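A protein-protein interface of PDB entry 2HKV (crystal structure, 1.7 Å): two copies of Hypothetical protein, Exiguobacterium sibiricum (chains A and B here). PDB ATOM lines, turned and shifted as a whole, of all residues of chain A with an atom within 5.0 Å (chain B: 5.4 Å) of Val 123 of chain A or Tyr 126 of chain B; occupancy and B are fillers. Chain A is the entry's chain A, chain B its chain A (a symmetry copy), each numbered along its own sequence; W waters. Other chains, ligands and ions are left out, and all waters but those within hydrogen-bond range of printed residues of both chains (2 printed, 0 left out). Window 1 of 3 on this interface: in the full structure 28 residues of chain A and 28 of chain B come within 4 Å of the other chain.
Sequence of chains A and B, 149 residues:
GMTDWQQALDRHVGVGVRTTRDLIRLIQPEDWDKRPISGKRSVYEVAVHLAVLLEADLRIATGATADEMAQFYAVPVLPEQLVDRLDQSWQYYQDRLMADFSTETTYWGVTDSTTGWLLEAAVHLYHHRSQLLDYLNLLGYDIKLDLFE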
ATOM      1  N   LEU A 119     -28.516  -2.883  18.607  1.00  0.00           N
ATOM      2  CA  LEU A 119     -27.817  -2.207  19.708  1.00  0.00           C
ATOM      3  C   LEU A 119     -28.546  -0.916  20.139  1.00  0.00           C
ATOM      4  O   LEU A 119     -28.627  -0.619  21.357  1.00  0.00           O
ATOM      5  CB  LEU A 119     -26.360  -1.902  19.349  1.00  0.00           C
ATOM      6  CG  LEU A 119     -25.518  -1.077  20.345  1.00  0.00           C
ATOM      7  CD1 LEU A 119     -25.493  -1.729  21.735  1.00  0.00           C
ATOM      8  CD2 LEU A 119     -24.102  -0.912  19.756  1.00  0.00           C
ATOM      9  N   GLU A 120     -29.099  -0.139  19.194  1.00  0.00           N
ATOM     10  CA  GLU A 120     -29.788   1.096  19.532  1.00  0.00           C
ATOM     11  C   GLU A 120     -30.951   0.821  20.459  1.00  0.00           C
ATOM     12  O   GLU A 120     -31.163   1.562  21.408  1.00  0.00           O
ATOM     13  CB  GLU A 120     -30.271   1.804  18.264  1.00  0.00           C
ATOM     14  CG  GLU A 120     -30.887   3.208  18.447  1.00  0.00           C
ATOM     15  CD  GLU A 120     -32.296   3.192  19.067  1.00  0.00           C
ATOM     16  OE1 GLU A 120     -33.023   2.204  18.846  1.00  0.00           O
ATOM     17  OE2 GLU A 120     -32.706   4.154  19.759  1.00  0.00           O
ATOM     18  N   ALA A 121     -31.664  -0.275  20.245  1.00  0.00           N
ATOM     19  CA  ALA A 121     -32.868  -0.518  21.016  1.00  0.00           C
ATOM     20  C   ALA A 121     -32.378  -0.911  22.414  1.00  0.00           C
ATOM     21  O   ALA A 121     -33.013  -0.559  23.396  1.00  0.00           O
ATOM     22  CB  ALA A 121     -33.683  -1.630  20.391  1.00  0.00           C
ATOM     23  N   ALA A 122     -31.278  -1.659  22.499  1.00  0.00           N
ATOM     24  CA  ALA A 122     -30.683  -2.040  23.792  1.00  0.00           C
ATOM     25  C   ALA A 122     -30.324  -0.808  24.688  1.00  0.00           C
ATOM     26  O   ALA A 122     -30.743  -0.692  25.849  1.00  0.00           O
ATOM     27  CB  ALA A 122     -29.442  -2.970  23.598  1.00  0.00           C
ATOM     28  N   VAL A 123     -29.545   0.110  24.142  1.00  0.00           N
ATOM     29  CA  VAL A 123     -29.149   1.289  24.891  1.00  0.00           C
ATOM     30  C   VAL A 123     -30.321   2.211  25.160  1.00  0.00           C
ATOM     31  O   VAL A 123     -30.346   2.870  26.182  1.00  0.00           O
ATOM     32  CB  VAL A 123     -27.947   2.069  24.226  1.00  0.00           C
ATOM     33  CG1 VAL A 123     -26.723   1.157  24.156  1.00  0.00           C
ATOM     34  CG2 VAL A 123     -28.278   2.626  22.842  1.00  0.00           C
ATOM     35  N   HIS A 124     -31.307   2.264  24.262  1.00  0.00           N
ATOM     36  CA  HIS A 124     -32.547   2.997  24.542  1.00  0.00           C
ATOM     37  C   HIS A 124     -33.332   2.418  25.742  1.00  0.00           C
ATOM     38  O   HIS A 124     -33.770   3.144  26.649  1.00  0.00           O
ATOM     39  CB  HIS A 124     -33.371   3.018  23.234  1.00  0.00           C
ATOM     40  CG  HIS A 124     -34.539   3.911  23.268  1.00  0.00           C
ATOM     41  ND1 HIS A 124     -35.546   3.823  22.347  1.00  0.00           N
ATOM     42  CD2 HIS A 124     -34.873   4.904  24.115  1.00  0.00           C
ATOM     43  CE1 HIS A 124     -36.455   4.731  22.620  1.00  0.00           C
ATOM     44  NE2 HIS A 124     -36.049   5.398  23.677  1.00  0.00           N
ATOM     45  N   LEU A 125     -33.354   1.101  25.840  1.00  0.00           N
ATOM     46  CA  LEU A 125     -33.931   0.421  26.982  1.00  0.00           C
ATOM     47  C   LEU A 125     -33.241   0.777  28.324  1.00  0.00           C
ATOM     48  O   LEU A 125     -33.922   1.158  29.314  1.00  0.00           O
ATOM     49  CB  LEU A 125     -33.953  -1.110  26.781  1.00  0.00           C
ATOM     50  CG  LEU A 125     -34.672  -1.899  27.885  1.00  0.00           C
ATOM     51  CD1 LEU A 125     -36.184  -1.797  27.743  1.00  0.00           C
ATOM     52  CD2 LEU A 125     -34.187  -3.392  27.850  1.00  0.00           C
ATOM     53  N   TYR A 126     -31.935   0.745  28.346  1.00  0.00           N
ATOM     54  CA  TYR A 126     -31.148   1.077  29.539  1.00  0.00           C
ATOM     55  C   TYR A 126     -31.270   2.550  29.866  1.00  0.00           C
ATOM     56  O   TYR A 126     -31.338   2.896  31.026  1.00  0.00           O
ATOM     57  CB  TYR A 126     -29.677   0.627  29.362  1.00  0.00           C
ATOM     58  CG  TYR A 126     -29.470  -0.835  29.767  1.00  0.00           C
ATOM     59  CD1 TYR A 126     -29.747  -1.871  28.853  1.00  0.00           C
ATOM     60  CD2 TYR A 126     -28.949  -1.167  30.993  1.00  0.00           C
ATOM     61  CE1 TYR A 126     -29.618  -3.199  29.185  1.00  0.00           C
ATOM     62  CE2 TYR A 126     -28.768  -2.490  31.344  1.00  0.00           C
ATOM     63  CZ  TYR A 126     -29.049  -3.503  30.421  1.00  0.00           C
ATOM     64  OH  TYR A 126     -28.859  -4.809  30.792  1.00  0.00           O
ATOM     65  N   HIS A 127     -31.373   3.424  28.867  1.00  0.00           N
ATOM     66  CA  HIS A 127     -31.661   4.860  29.101  1.00  0.00           C
ATOM     67  C   HIS A 127     -32.957   5.044  29.927  1.00  0.00           C
ATOM     68  O   HIS A 127     -32.988   5.742  30.929  1.00  0.00           O
ATOM     69  CB  HIS A 127     -31.745   5.591  27.751  1.00  0.00           C
ATOM     70  CG  HIS A 127     -32.207   7.025  27.830  1.00  0.00           C
ATOM     71  ND1 HIS A 127     -31.364   8.056  28.188  1.00  0.00           N
ATOM     72  CD2 HIS A 127     -33.425   7.584  27.627  1.00  0.00           C
ATOM     73  CE1 HIS A 127     -32.037   9.200  28.175  1.00  0.00           C
ATOM     74  NE2 HIS A 127     -33.295   8.945  27.850  1.00  0.00           N
ATOM     75  N   HIS B  12     -22.565   3.887  18.477  1.00  0.00           N
ATOM     76  CA  HIS B  12     -23.468   4.136  19.587  1.00  0.00           C
ATOM     77  C   HIS B  12     -22.740   4.491  20.854  1.00  0.00           C
ATOM     78  O   HIS B  12     -23.184   5.383  21.608  1.00  0.00           O
ATOM     79  CB  HIS B  12     -24.473   2.960  19.734  1.00  0.00           C
ATOM     80  CG  HIS B  12     -25.436   2.876  18.592  1.00  0.00           C
ATOM     81  ND1 HIS B  12     -26.568   3.685  18.515  1.00  0.00           N
ATOM     82  CD2 HIS B  12     -25.416   2.152  17.450  1.00  0.00           C
ATOM     83  CE1 HIS B  12     -27.172   3.464  17.360  1.00  0.00           C
ATOM     84  NE2 HIS B  12     -26.493   2.559  16.684  1.00  0.00           N
ATOM     85  N   VAL B  13     -21.592   3.876  21.122  1.00  0.00           N
ATOM     86  CA  VAL B  13     -20.808   4.326  22.266  1.00  0.00           C
ATOM     87  C   VAL B  13     -20.211   5.724  21.995  1.00  0.00           C
ATOM     88  O   VAL B  13     -20.159   6.578  22.874  1.00  0.00           O
ATOM     89  CB  VAL B  13     -19.699   3.328  22.731  1.00  0.00           C
ATOM     90  CG1 VAL B  13     -18.994   3.918  23.944  1.00  0.00           C
ATOM     91  CG2 VAL B  13     -20.267   1.967  23.099  1.00  0.00           C
ATOM     92  N   VAL B  15     -21.675   8.119  20.300  1.00  0.00           N
ATOM     93  CA  VAL B  15     -22.767   9.054  20.576  1.00  0.00           C
ATOM     94  C   VAL B  15     -22.866   9.279  22.057  1.00  0.00           C
ATOM     95  O   VAL B  15     -23.014  10.413  22.517  1.00  0.00           O
ATOM     96  CB  VAL B  15     -24.192   8.546  20.119  1.00  0.00           C
ATOM     97  CG1 VAL B  15     -25.300   9.434  20.676  1.00  0.00           C
ATOM     98  CG2 VAL B  15     -24.328   8.407  18.562  1.00  0.00           C
ATOM     99  N   GLY B  16     -22.895   8.172  22.798  1.00  0.00           N
ATOM    100  CA  GLY B  16     -22.892   8.211  24.258  1.00  0.00           C
ATOM    101  C   GLY B  16     -21.817   9.107  24.817  1.00  0.00           C
ATOM    102  O   GLY B  16     -22.065   9.918  25.708  1.00  0.00           O
ATOM    103  N   ALA B 121     -20.304  -2.366  28.967  1.00  0.00           N
ATOM    104  CA  ALA B 121     -19.760  -1.066  29.311  1.00  0.00           C
ATOM    105  C   ALA B 121     -20.637  -0.054  28.565  1.00  0.00           C
ATOM    106  O   ALA B 121     -20.894   1.020  29.086  1.00  0.00           O
ATOM    107  CB  ALA B 121     -18.315  -0.963  28.873  1.00  0.00           C
ATOM    108  N   ALA B 122     -21.064  -0.382  27.345  1.00  0.00           N
ATOM    109  CA  ALA B 122     -21.964   0.486  26.566  1.00  0.00           C
ATOM    110  C   ALA B 122     -23.299   0.815  27.316  1.00  0.00           C
ATOM    111  O   ALA B 122     -23.680   1.979  27.504  1.00  0.00           O
ATOM    112  CB  ALA B 122     -22.250  -0.110  25.150  1.00  0.00           C
ATOM    113  N   VAL B 123     -24.005  -0.218  27.740  1.00  0.00           N
ATOM    114  CA  VAL B 123     -25.262  -0.022  28.441  1.00  0.00           C
ATOM    115  C   VAL B 123     -25.059   0.606  29.805  1.00  0.00           C
ATOM    116  O   VAL B 123     -25.908   1.347  30.258  1.00  0.00           O
ATOM    117  CB  VAL B 123     -26.128  -1.339  28.539  1.00  0.00           C
ATOM    118  CG1 VAL B 123     -26.477  -1.827  27.133  1.00  0.00           C
ATOM    119  CG2 VAL B 123     -25.449  -2.452  29.338  1.00  0.00           C
ATOM    120  N   HIS B 124     -23.933   0.332  30.469  1.00  0.00           N
ATOM    121  CA  HIS B 124     -23.595   1.040  31.708  1.00  0.00           C
ATOM    122  C   HIS B 124     -23.398   2.559  31.500  1.00  0.00           C
ATOM    123  O   HIS B 124     -23.937   3.397  32.241  1.00  0.00           O
ATOM    124  CB  HIS B 124     -22.349   0.346  32.307  1.00  0.00           C
ATOM    125  CG  HIS B 124     -22.011   0.779  33.670  1.00  0.00           C
ATOM    126  ND1 HIS B 124     -20.790   0.523  34.231  1.00  0.00           N
ATOM    127  CD2 HIS B 124     -22.723   1.460  34.588  1.00  0.00           C
ATOM    128  CE1 HIS B 124     -20.762   1.026  35.443  1.00  0.00           C
ATOM    129  NE2 HIS B 124     -21.931   1.581  35.673  1.00  0.00           N
ATOM    130  N   LEU B 125     -22.776   2.917  30.391  1.00  0.00           N
ATOM    131  CA  LEU B 125     -22.642   4.304  29.994  1.00  0.00           C
ATOM    132  C   LEU B 125     -24.000   5.018  29.780  1.00  0.00           C
ATOM    133  O   LEU B 125     -24.244   6.117  30.349  1.00  0.00           O
ATOM    134  CB  LEU B 125     -21.754   4.452  28.737  1.00  0.00           C
ATOM    135  CG  LEU B 125     -21.447   5.900  28.327  1.00  0.00           C
ATOM    136  CD1 LEU B 125     -20.384   6.516  29.226  1.00  0.00           C
ATOM    137  CD2 LEU B 125     -21.016   5.928  26.819  1.00  0.00           C
ATOM    138  N   TYR B 126     -24.893   4.392  29.062  1.00  0.00           N
ATOM    139  CA  TYR B 126     -26.229   4.936  28.795  1.00  0.00           C
ATOM    140  C   TYR B 126     -27.054   4.978  30.063  1.00  0.00           C
ATOM    141  O   TYR B 126     -27.790   5.920  30.261  1.00  0.00           O
ATOM    142  CB  TYR B 126     -26.923   4.143  27.660  1.00  0.00           C
ATOM    143  CG  TYR B 126     -26.548   4.673  26.274  1.00  0.00           C
ATOM    144  CD1 TYR B 126     -25.358   4.249  25.649  1.00  0.00           C
ATOM    145  CD2 TYR B 126     -27.386   5.512  25.582  1.00  0.00           C
ATOM    146  CE1 TYR B 126     -24.957   4.730  24.424  1.00  0.00           C
ATOM    147  CE2 TYR B 126     -27.033   5.982  24.333  1.00  0.00           C
ATOM    148  CZ  TYR B 126     -25.848   5.548  23.731  1.00  0.00           C
ATOM    149  OH  TYR B 126     -25.521   6.028  22.488  1.00  0.00           O
ATOM    150  N   HIS B 127     -26.893   4.012  30.966  1.00  0.00           N
ATOM    151  CA  HIS B 127     -27.537   4.066  32.302  1.00  0.00           C
ATOM    152  C   HIS B 127     -27.173   5.372  33.046  1.00  0.00           C
ATOM    153  O   HIS B 127     -28.027   6.092  33.539  1.00  0.00           O
ATOM    154  CB  HIS B 127     -27.133   2.823  33.112  1.00  0.00           C
ATOM    155  CG  HIS B 127     -27.574   2.834  34.556  1.00  0.00           C
ATOM    156  ND1 HIS B 127     -28.857   2.507  34.940  1.00  0.00           N
ATOM    157  CD2 HIS B 127     -26.908   3.159  35.691  1.00  0.00           C
ATOM    158  CE1 HIS B 127     -28.958   2.603  36.260  1.00  0.00           C
ATOM    159  NE2 HIS B 127     -27.795   3.009  36.744  1.00  0.00           N
ATOM    160  N   HIS B 128     -25.879   5.664  33.156  1.00  0.00           N
ATOM    161  CA  HIS B 128     -25.489   6.820  33.890  1.00  0.00           C
ATOM    162  C   HIS B 128     -25.607   8.119  33.133  1.00  0.00           C
ATOM    163  O   HIS B 128     -25.787   9.157  33.791  1.00  0.00           O
ATOM    164  CB  HIS B 128     -24.097   6.685  34.499  1.00  0.00           C
ATOM    165  CG  HIS B 128     -24.000   5.640  35.553  1.00  0.00           C
ATOM    166  ND1 HIS B 128     -24.649   5.747  36.766  1.00  0.00           N
ATOM    167  CD2 HIS B 128     -23.283   4.504  35.600  1.00  0.00           C
ATOM    168  CE1 HIS B 128     -24.314   4.695  37.510  1.00  0.00           C
ATOM    169  NE2 HIS B 128     -23.545   3.887  36.796  1.00  0.00           N
ATOM    170  N   ARG B 129     -25.529   8.122  31.801  1.00  0.00           N
ATOM    171  CA  ARG B 129     -25.807   9.338  31.037  1.00  0.00           C
ATOM    172  C   ARG B 129     -27.249   9.793  31.346  1.00  0.00           C
ATOM    173  O   ARG B 129     -27.554  10.996  31.555  1.00  0.00           O
ATOM    174  CB  ARG B 129     -25.682   9.084  29.563  1.00  0.00           C
ATOM    175  CG  ARG B 129     -25.780  10.366  28.719  1.00  0.00           C
ATOM    176  CD  ARG B 129     -25.838  10.117  27.216  1.00  0.00           C
ATOM    177  NE  ARG B 129     -27.084   9.444  26.834  1.00  0.00           N
ATOM    178  CZ  ARG B 129     -27.599   9.466  25.613  1.00  0.00           C
ATOM    179  NH1 ARG B 129     -26.973  10.073  24.628  1.00  0.00           N
ATOM    180  NH2 ARG B 129     -28.720   8.802  25.382  1.00  0.00           N
ATOM    181  N   SER B 130     -28.173   8.822  31.384  1.00  0.00           N
ATOM    182  CA  SER B 130     -29.578   9.099  31.738  1.00  0.00           C
ATOM    183  C   SER B 130     -29.696   9.701  33.133  1.00  0.00           C
ATOM    184  O   SER B 130     -30.449  10.712  33.355  1.00  0.00           O
ATOM    185  CB  SER B 130     -30.411   7.821  31.658  1.00  0.00           C
ATOM    186  OG  SER B 130     -31.796   8.113  31.756  1.00  0.00           O
ATOM    187  N   GLN B 131     -28.979   9.116  34.092  1.00  0.00           N
ATOM    188  CA  GLN B 131     -28.988   9.635  35.462  1.00  0.00           C
ATOM    189  C   GLN B 131     -28.563  11.111  35.471  1.00  0.00           C
ATOM    190  O   GLN B 131     -29.234  11.966  36.122  1.00  0.00           O
ATOM    191  CB  GLN B 131     -28.017   8.853  36.305  1.00  0.00           C
ATOM    192  CG  GLN B 131     -28.082   9.142  37.758  1.00  0.00           C
ATOM    193  CD  GLN B 131     -27.258   8.164  38.575  1.00  0.00           C
ATOM    194  OE1 GLN B 131     -26.607   7.274  38.030  1.00  0.00           O
ATOM    195  NE2 GLN B 131     -27.305   8.312  39.920  1.00  0.00           N
ATOM    196  N   LEU B 147     -30.198  13.199  22.075  1.00  0.00           N
ATOM    197  CA  LEU B 147     -29.563  12.082  22.797  1.00  0.00           C
ATOM    198  C   LEU B 147     -29.459  10.788  21.974  1.00  0.00           C
ATOM    199  O   LEU B 147     -28.734   9.860  22.339  1.00  0.00           O
ATOM    200  CB  LEU B 147     -30.344  11.788  24.094  1.00  0.00           C
ATOM    201  CG  LEU B 147     -30.575  12.935  25.092  1.00  0.00           C
ATOM    202  CD1 LEU B 147     -31.462  12.395  26.187  1.00  0.00           C
ATOM    203  CD2 LEU B 147     -29.276  13.507  25.655  1.00  0.00           C
ATOM    204  N   PHE B 148     -30.226  10.728  20.890  1.00  0.00           N
ATOM    205  CA  PHE B 148     -30.170   9.637  19.924  1.00  0.00           C
ATOM    206  C   PHE B 148     -30.234  10.278  18.534  1.00  0.00           C
ATOM    207  O   PHE B 148     -30.040   9.616  17.512  1.00  0.00           O
ATOM    208  CB  PHE B 148     -31.343   8.659  20.133  1.00  0.00           C
ATOM    209  CG  PHE B 148     -31.280   7.867  21.436  1.00  0.00           C
ATOM    210  CD1 PHE B 148     -30.595   6.638  21.501  1.00  0.00           C
ATOM    211  CD2 PHE B 148     -31.924   8.345  22.598  1.00  0.00           C
ATOM    212  CE1 PHE B 148     -30.554   5.921  22.687  1.00  0.00           C
ATOM    213  CE2 PHE B 148     -31.878   7.627  23.784  1.00  0.00           C
ATOM    214  CZ  PHE B 148     -31.189   6.422  23.839  1.00  0.00           C
HETATM  215  O   HOH W   1     -28.616   7.558  28.187  1.00  0.00           O
HETATM  216  O   HOH W   2     -30.497   1.232  33.073  1.00  0.00           O
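NH1 of Arg 129 of chain B is in hydrogen-bond range of O of Leu 147 of chain B (2.9 Å). The backbone carbonyl oxygen (O) of His 12 of chain B lies within hydrogen-bond range of the side-chain hydroxyl (OH) of Tyr 126 of chain B. The side-chain hydroxyl of Tyr 126 of chain B sits at hydrogen-bond distance from the backbone NH of Gly 16 of chain B.
Water W1 lies within hydrogen-bond range of O of Tyr 126 of chain B (2.8 Å), NE of Arg 129 of chain B (2.8 Å), ND1 of His 127 of chain A (2.8 Å) and N of Ser 130 of chain B (3.5 Å). Water W2 lies within hydrogen-bond range of the backbone carbonyl oxygen (O) of Tyr 126 of chain A (2.8 Å) and a ring nitrogen (ND1) of His 127 of chain B (2.8 Å).
Val 123 of chain A touches Tyr 126 of chain B, and with the chains exchanged Tyr 126 of chain A touches Val 123 of chain B. 7 positions are printed for both chains.
Of the 9 printed residues of chain A, 6 touch a printed residue of chain B. Hydrophobic or aromatic side chains of chain B within 4 Å of the printed part of chain A: His 12, Val 123, Tyr 126, Leu 147 and Phe 148. Among the printed residues, no Asp or Glu carboxylate lies within 4 Å of a Lys or Arg side-chain nitrogen of the other chain.
O of His 127 of chain A lies within hydrogen-bond range of OG of Ser 130 of chain B (2.8 Å).
Printed residues of chain B within 4 Å of Leu 119 of chain A: His 12 (3.9 Å). Of the printed residues of chain B, Val 123 of chain A touches Tyr 126 (3.6 Å). Of the printed residues of chain B, His 127 of chain A touches Arg 129, Ser 130 and Leu 147. Of the printed residues of chain A, His 12 of chain B touches Leu 119 and Glu 120. Tyr 126 of chain B touches one residue of chain A. Of the printed residues of chain A, Leu 147 of chain B touches His 127. Of the printed residues of chain A, Phe 148 of chain B touches Glu 120 and His 124. The nearest printed residue of chain B that does not touch Val 123 of chain A is Phe 148 of chain B (4.01 Å). The nearest residue of chain A that does not touch Tyr 126 of chain B is His 127 of chain A (4.2 Å). The nearest printed residue of chain B that does not touch Tyr 126 of chain A is His 127 of chain B (4.2 Å).
His 12 of chain B touches Leu 119 of chain A. CE1 of His 12 of chain B touches CB of Glu 120 of chain A, at 3.6 Å. Glu 120 of chain A touches Phe 148 of chain B. Val 123 of chain A touches Tyr 126 of chain B (CB to CG, 3.6 Å). His 124 of chain A touches Phe 148 of chain B (CA to CZ, 3.8 Å). CG of Tyr 126 of chain A touches CB of Val 123 of chain B, at 3.6 Å. Arg 129 of chain B touches His 127 of chain A. CE1 of His 127 of chain A touches CD1 of Leu 147 of chain B, 3.8 Å away.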
